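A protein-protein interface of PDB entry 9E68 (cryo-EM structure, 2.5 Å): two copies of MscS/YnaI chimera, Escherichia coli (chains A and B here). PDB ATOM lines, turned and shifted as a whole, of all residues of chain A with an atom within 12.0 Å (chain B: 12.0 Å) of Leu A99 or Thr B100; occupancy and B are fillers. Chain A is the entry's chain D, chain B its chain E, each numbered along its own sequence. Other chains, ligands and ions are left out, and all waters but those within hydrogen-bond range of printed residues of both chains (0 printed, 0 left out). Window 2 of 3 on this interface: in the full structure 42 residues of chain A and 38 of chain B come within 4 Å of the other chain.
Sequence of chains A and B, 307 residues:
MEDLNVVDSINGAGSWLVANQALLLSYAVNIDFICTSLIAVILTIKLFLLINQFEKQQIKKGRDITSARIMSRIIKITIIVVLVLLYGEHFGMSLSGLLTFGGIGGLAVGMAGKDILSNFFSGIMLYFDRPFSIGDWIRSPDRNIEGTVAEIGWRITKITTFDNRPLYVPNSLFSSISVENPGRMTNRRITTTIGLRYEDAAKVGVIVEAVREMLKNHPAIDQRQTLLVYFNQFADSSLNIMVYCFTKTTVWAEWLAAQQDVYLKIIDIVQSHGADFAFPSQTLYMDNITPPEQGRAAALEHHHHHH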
ATOM      1  N   GLY A  97      20.926 -29.542  16.911  1.00  0.00           N
ATOM      2  CA  GLY A  97      21.971 -28.969  17.739  1.00  0.00           C
ATOM      3  C   GLY A  97      22.428 -27.603  17.268  1.00  0.00           C
ATOM      4  O   GLY A  97      22.624 -26.691  18.074  1.00  0.00           O
ATOM      5  N   LEU A  98      22.605 -27.463  15.952  1.00  0.00           N
ATOM      6  CA  LEU A  98      23.041 -26.185  15.398  1.00  0.00           C
ATOM      7  C   LEU A  98      22.013 -25.091  15.654  1.00  0.00           C
ATOM      8  O   LEU A  98      22.370 -23.971  16.040  1.00  0.00           O
ATOM      9  CB  LEU A  98      23.307 -26.328  13.900  1.00  0.00           C
ATOM     10  CG  LEU A  98      24.746 -26.633  13.478  1.00  0.00           C
ATOM     11  CD1 LEU A  98      24.930 -26.382  11.988  1.00  0.00           C
ATOM     12  CD2 LEU A  98      25.734 -25.808  14.289  1.00  0.00           C
ATOM     13  N   LEU A  99      20.728 -25.400  15.455  1.00  0.00           N
ATOM     14  CA  LEU A  99      19.685 -24.395  15.636  1.00  0.00           C
ATOM     15  C   LEU A  99      19.623 -23.919  17.082  1.00  0.00           C
ATOM     16  O   LEU A  99      19.578 -22.712  17.344  1.00  0.00           O
ATOM     17  CB  LEU A  99      18.335 -24.961  15.185  1.00  0.00           C
ATOM     18  CG  LEU A  99      17.068 -24.104  15.290  1.00  0.00           C
ATOM     19  CD1 LEU A  99      16.107 -24.471  14.172  1.00  0.00           C
ATOM     20  CD2 LEU A  99      16.378 -24.277  16.638  1.00  0.00           C
ATOM     21  N   THR A 100      19.634 -24.852  18.038  1.00  0.00           N
ATOM     22  CA  THR A 100      19.545 -24.456  19.438  1.00  0.00           C
ATOM     23  C   THR A 100      20.820 -23.768  19.913  1.00  0.00           C
ATOM     24  O   THR A 100      20.749 -22.841  20.727  1.00  0.00           O
ATOM     25  CB  THR A 100      19.216 -25.666  20.320  1.00  0.00           C
ATOM     26  OG1 THR A 100      19.148 -25.255  21.690  1.00  0.00           O
ATOM     27  CG2 THR A 100      20.259 -26.763  20.169  1.00  0.00           C
ATOM     28  N   PHE A 101      21.987 -24.188  19.415  1.00  0.00           N
ATOM     29  CA  PHE A 101      23.227 -23.501  19.765  1.00  0.00           C
ATOM     30  C   PHE A 101      23.220 -22.065  19.254  1.00  0.00           C
ATOM     31  O   PHE A 101      23.597 -21.133  19.979  1.00  0.00           O
ATOM     32  CB  PHE A 101      24.425 -24.269  19.208  1.00  0.00           C
ATOM     33  CG  PHE A 101      25.748 -23.626  19.505  1.00  0.00           C
ATOM     34  CD1 PHE A 101      26.174 -23.458  20.813  1.00  0.00           C
ATOM     35  CD2 PHE A 101      26.567 -23.190  18.477  1.00  0.00           C
ATOM     36  CE1 PHE A 101      27.391 -22.866  21.089  1.00  0.00           C
ATOM     37  CE2 PHE A 101      27.786 -22.597  18.747  1.00  0.00           C
ATOM     38  CZ  PHE A 101      28.199 -22.435  20.055  1.00  0.00           C
ATOM     39  N   GLY A 102      22.793 -21.868  18.005  1.00  0.00           N
ATOM     40  CA  GLY A 102      22.692 -20.520  17.474  1.00  0.00           C
ATOM     41  C   GLY A 102      21.682 -19.676  18.225  1.00  0.00           C
ATOM     42  O   GLY A 102      21.913 -18.491  18.473  1.00  0.00           O
ATOM     43  N   GLY A 103      20.549 -20.275  18.597  1.00  0.00           N
ATOM     44  CA  GLY A 103      19.568 -19.549  19.386  1.00  0.00           C
ATOM     45  C   GLY A 103      20.104 -19.138  20.744  1.00  0.00           C
ATOM     46  O   GLY A 103      19.857 -18.023  21.206  1.00  0.00           O
ATOM     47  N   ILE A 104      20.849 -20.032  21.397  1.00  0.00           N
ATOM     48  CA  ILE A 104      21.443 -19.712  22.693  1.00  0.00           C
ATOM     49  C   ILE A 104      22.438 -18.568  22.555  1.00  0.00           C
ATOM     50  O   ILE A 104      22.431 -17.610  23.341  1.00  0.00           O
ATOM     51  CB  ILE A 104      22.108 -20.962  23.295  1.00  0.00           C
ATOM     52  N   GLY A 105      23.315 -18.656  21.552  1.00  0.00           N
ATOM     53  CA  GLY A 105      24.284 -17.593  21.338  1.00  0.00           C
ATOM     54  C   GLY A 105      23.624 -16.262  21.036  1.00  0.00           C
ATOM     55  O   GLY A 105      24.031 -15.221  21.560  1.00  0.00           O
ATOM     56  N   GLY A 106      22.586 -16.279  20.198  1.00  0.00           N
ATOM     57  CA  GLY A 106      21.884 -15.049  19.880  1.00  0.00           C
ATOM     58  C   GLY A 106      21.154 -14.464  21.072  1.00  0.00           C
ATOM     59  O   GLY A 106      21.118 -13.245  21.246  1.00  0.00           O
ATOM     60  N   LEU A 107      20.556 -15.319  21.905  1.00  0.00           N
ATOM     61  CA  LEU A 107      19.900 -14.835  23.113  1.00  0.00           C
ATOM     62  C   LEU A 107      20.909 -14.178  24.045  1.00  0.00           C
ATOM     63  O   LEU A 107      20.650 -13.098  24.592  1.00  0.00           O
ATOM     64  CB  LEU A 107      19.169 -15.993  23.802  1.00  0.00           C
ATOM     65  CG  LEU A 107      18.326 -15.861  25.082  1.00  0.00           C
ATOM     66  CD1 LEU A 107      17.574 -17.161  25.310  1.00  0.00           C
ATOM     67  CD2 LEU A 107      19.139 -15.529  26.331  1.00  0.00           C
ATOM     68  N   ALA A 108      22.071 -14.811  24.227  1.00  0.00           N
ATOM     69  CA  ALA A 108      23.103 -14.226  25.077  1.00  0.00           C
ATOM     70  C   ALA A 108      23.574 -12.886  24.523  1.00  0.00           C
ATOM     71  O   ALA A 108      23.725 -11.909  25.267  1.00  0.00           O
ATOM     72  CB  ALA A 108      24.277 -15.196  25.220  1.00  0.00           C
ATOM     73  N   VAL A 109      23.798 -12.820  23.207  1.00  0.00           N
ATOM     74  CA  VAL A 109      24.278 -11.585  22.593  1.00  0.00           C
ATOM     75  C   VAL A 109      23.239 -10.477  22.729  1.00  0.00           C
ATOM     76  O   VAL A 109      23.570  -9.334  23.066  1.00  0.00           O
ATOM     77  CB  VAL A 109      24.654 -11.836  21.120  1.00  0.00           C
ATOM     78  CG1 VAL A 109      24.711 -10.526  20.347  1.00  0.00           C
ATOM     79  CG2 VAL A 109      25.983 -12.571  21.032  1.00  0.00           C
ATOM     80  N   GLY A 110      21.969 -10.798  22.476  1.00  0.00           N
ATOM     81  CA  GLY A 110      20.927  -9.791  22.580  1.00  0.00           C
ATOM     82  C   GLY A 110      20.729  -9.293  23.998  1.00  0.00           C
ATOM     83  O   GLY A 110      20.524  -8.097  24.221  1.00  0.00           O
ATOM     84  N   MET A 111      20.784 -10.199  24.977  1.00  0.00           N
ATOM     85  CA  MET A 111      20.659  -9.783  26.368  1.00  0.00           C
ATOM     86  C   MET A 111      21.847  -8.956  26.836  1.00  0.00           C
ATOM     87  O   MET A 111      21.659  -8.005  27.603  1.00  0.00           O
ATOM     88  CB  MET A 111      20.489 -11.005  27.272  1.00  0.00           C
ATOM     89  CG  MET A 111      19.043 -11.407  27.504  1.00  0.00           C
ATOM     90  SD  MET A 111      17.974  -9.977  27.747  1.00  0.00           S
ATOM     91  CE  MET A 111      16.825 -10.617  28.961  1.00  0.00           C
ATOM     92  N   GLY B  97      20.589 -21.672   9.909  1.00  0.00           N
ATOM     93  CA  GLY B  97      21.403 -20.519  10.243  1.00  0.00           C
ATOM     94  C   GLY B  97      20.688 -19.198  10.031  1.00  0.00           C
ATOM     95  O   GLY B  97      20.770 -18.296  10.865  1.00  0.00           O
ATOM     96  N   LEU B  98      19.986 -19.086   8.901  1.00  0.00           N
ATOM     97  CA  LEU B  98      19.256 -17.857   8.606  1.00  0.00           C
ATOM     98  C   LEU B  98      18.164 -17.602   9.637  1.00  0.00           C
ATOM     99  O   LEU B  98      17.997 -16.470  10.108  1.00  0.00           O
ATOM    100  CB  LEU B  98      18.660 -17.928   7.200  1.00  0.00           C
ATOM    101  CG  LEU B  98      19.487 -17.322   6.064  1.00  0.00           C
ATOM    102  CD1 LEU B  98      18.632 -17.137   4.821  1.00  0.00           C
ATOM    103  CD2 LEU B  98      20.109 -16.002   6.492  1.00  0.00           C
ATOM    104  N   LEU B  99      17.415 -18.645  10.004  1.00  0.00           N
ATOM    105  CA  LEU B  99      16.320 -18.474  10.954  1.00  0.00           C
ATOM    106  C   LEU B  99      16.832 -18.029  12.318  1.00  0.00           C
ATOM    107  O   LEU B  99      16.289 -17.094  12.919  1.00  0.00           O
ATOM    108  CB  LEU B  99      15.519 -19.775  11.064  1.00  0.00           C
ATOM    109  CG  LEU B  99      14.317 -19.862  12.013  1.00  0.00           C
ATOM    110  CD1 LEU B  99      13.284 -20.818  11.444  1.00  0.00           C
ATOM    111  CD2 LEU B  99      14.729 -20.319  13.406  1.00  0.00           C
ATOM    112  N   THR B 100      17.889 -18.676  12.820  1.00  0.00           N
ATOM    113  CA  THR B 100      18.405 -18.309  14.134  1.00  0.00           C
ATOM    114  C   THR B 100      19.093 -16.949  14.111  1.00  0.00           C
ATOM    115  O   THR B 100      19.000 -16.198  15.089  1.00  0.00           O
ATOM    116  CB  THR B 100      19.351 -19.393  14.661  1.00  0.00           C
ATOM    117  OG1 THR B 100      19.846 -19.009  15.950  1.00  0.00           O
ATOM    118  CG2 THR B 100      20.520 -19.620  13.716  1.00  0.00           C
ATOM    119  N   PHE B 101      19.769 -16.603  13.012  1.00  0.00           N
ATOM    120  CA  PHE B 101      20.358 -15.272  12.898  1.00  0.00           C
ATOM    121  C   PHE B 101      19.280 -14.194  12.905  1.00  0.00           C
ATOM    122  O   PHE B 101      19.412 -13.169  13.589  1.00  0.00           O
ATOM    123  CB  PHE B 101      21.205 -15.183  11.628  1.00  0.00           C
ATOM    124  CG  PHE B 101      21.855 -13.846  11.425  1.00  0.00           C
ATOM    125  CD1 PHE B 101      22.767 -13.357  12.345  1.00  0.00           C
ATOM    126  CD2 PHE B 101      21.553 -13.077  10.314  1.00  0.00           C
ATOM    127  CE1 PHE B 101      23.367 -12.125  12.160  1.00  0.00           C
ATOM    128  CE2 PHE B 101      22.149 -11.845  10.124  1.00  0.00           C
ATOM    129  CZ  PHE B 101      23.057 -11.369  11.048  1.00  0.00           C
ATOM    130  N   GLY B 102      18.200 -14.413  12.151  1.00  0.00           N
ATOM    131  CA  GLY B 102      17.099 -13.466  12.163  1.00  0.00           C
ATOM    132  C   GLY B 102      16.441 -13.360  13.524  1.00  0.00           C
ATOM    133  O   GLY B 102      16.076 -12.269  13.962  1.00  0.00           O
ATOM    134  N   GLY B 103      16.281 -14.495  14.210  1.00  0.00           N
ATOM    135  CA  GLY B 103      15.726 -14.459  15.553  1.00  0.00           C
ATOM    136  C   GLY B 103      16.598 -13.686  16.523  1.00  0.00           C
ATOM    137  O   GLY B 103      16.097 -12.918  17.345  1.00  0.00           O
ATOM    138  N   ILE B 104      17.917 -13.873  16.432  1.00  0.00           N
ATOM    139  CA  ILE B 104      18.839 -13.143  17.299  1.00  0.00           C
ATOM    140  C   ILE B 104      18.748 -11.646  17.031  1.00  0.00           C
ATOM    141  O   ILE B 104      18.647 -10.833  17.960  1.00  0.00           O
ATOM    142  CB  ILE B 104      20.275 -13.660  17.103  1.00  0.00           C
ATOM    143  N   GLY B 105      18.780 -11.263  15.752  1.00  0.00           N
ATOM    144  CA  GLY B 105      18.679  -9.853  15.413  1.00  0.00           C
ATOM    145  C   GLY B 105      17.370  -9.239  15.870  1.00  0.00           C
ATOM    146  O   GLY B 105      17.346  -8.127  16.404  1.00  0.00           O
ATOM    147  N   GLY B 106      16.265  -9.963  15.680  1.00  0.00           N
ATOM    148  CA  GLY B 106      14.975  -9.449  16.100  1.00  0.00           C
ATOM    149  C   GLY B 106      14.849  -9.324  17.606  1.00  0.00           C
ATOM    150  O   GLY B 106      14.272  -8.356  18.107  1.00  0.00           O
ATOM    151  N   LEU B 107      15.374 -10.301  18.348  1.00  0.00           N
ATOM    152  CA  LEU B 107      15.350 -10.207  19.804  1.00  0.00           C
ATOM    153  C   LEU B 107      16.175  -9.020  20.279  1.00  0.00           C
ATOM    154  O   LEU B 107      15.759  -8.286  21.184  1.00  0.00           O
ATOM    155  CB  LEU B 107      15.852 -11.513  20.423  1.00  0.00           C
ATOM    156  CG  LEU B 107      16.491 -11.519  21.816  1.00  0.00           C
ATOM    157  CD1 LEU B 107      15.544 -10.970  22.882  1.00  0.00           C
ATOM    158  CD2 LEU B 107      16.942 -12.922  22.178  1.00  0.00           C
ATOM    159  N   ALA B 108      17.346  -8.807  19.672  1.00  0.00           N
ATOM    160  CA  ALA B 108      18.167  -7.655  20.035  1.00  0.00           C
ATOM    161  C   ALA B 108      17.437  -6.348  19.746  1.00  0.00           C
ATOM    162  O   ALA B 108      17.451  -5.420  20.564  1.00  0.00           O
ATOM    163  CB  ALA B 108      19.501  -7.707  19.290  1.00  0.00           C
ATOM    164  N   VAL B 109      16.784  -6.263  18.584  1.00  0.00           N
ATOM    165  CA  VAL B 109      16.064  -5.044  18.222  1.00  0.00           C
ATOM    166  C   VAL B 109      14.909  -4.795  19.184  1.00  0.00           C
ATOM    167  O   VAL B 109      14.697  -3.666  19.645  1.00  0.00           O
ATOM    168  CB  VAL B 109      15.579  -5.126  16.761  1.00  0.00           C
ATOM    169  CG1 VAL B 109      14.475  -4.112  16.503  1.00  0.00           C
ATOM    170  CG2 VAL B 109      16.743  -4.906  15.808  1.00  0.00           C
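The backbone NH of Gly A103 sits at hydrogen-bond distance from the side-chain hydroxyl of Thr B100, 3.0 Å away.
The backbone carbonyl oxygen (O) of Gly A102 sits close to the side-chain hydroxyl (OG1) of Thr B100, at 3.3 Å.
Leu A99 touches Thr B100.
Gly A106 touches Ile B104.
CA of Leu A107 touches CD2 of Leu B107 (3.6 Å).
No residue of chain B comes within 4 Å of Gly A97.
Of chain B, only Thr B100 comes within 4 Å of Leu A99.
Of chain B, only Thr B100 comes within 4 Å of Gly A102.
Gly A105 touches none of the printed residues of chain B.
Gly A106 touches one residue of chain B.
Of the printed residues of chain B, Leu A107 touches Leu B107.
Gly A110 touches none of the printed residues of chain B.
No residue of chain A comes within 4 Å of Leu B99.
Thr B100 touches just these residues of chain A: Leu A99, Gly A102 and Gly A103.
No residue of chain A comes within 4 Å of Phe B101.
Ile B104 touches one residue of chain A.
Of the printed residues of chain A, Leu B107 touches Leu A107.
The nearest residue of chain B that does not touch Leu A99 is Leu B99 (4.4 Å).
The nearest residue of chain A that does not touch Thr B100 is Leu A98 (5.3 Å).
Of the 13 printed residues of chain B, 3 touch a printed residue of chain A.
Hydrophobic or aromatic side chains of chain B that line the printed part of chain A: Ile B104 and Leu B107.
Along chain B the printed residues that touch a printed residue of chain A span positions 100 to 107.
Of the 15 printed residues of chain A, 5 touch a printed residue of chain B.
Printed residues of chain A that touch a printed residue of chain B: Leu A99, Gly A102, Gly A103, Gly A106 and Leu A107.
Among the printed residues, no Asp or Glu carboxylate lies within 4 Å of a Lys or Arg side-chain nitrogen of the other chain.
Leu A99 touches Thr B100, but with the chains exchanged Thr A100 does not touch Leu B99 (8.1 Å).
Gly A102 touches Thr B100, but with the chains exchanged Thr A100 does not touch Gly B102 (12.1 Å).
Gly A103 touches Thr B100, but with the chains exchanged Thr A100 does not touch Gly B103 (10.9 Å).
Leu B107 touches its own counterpart, Leu A107.
Positions printed for both chains: 97, 98, 99, 100, 101, 102, 103, 104, 105, 106, 107, 108 and 109.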
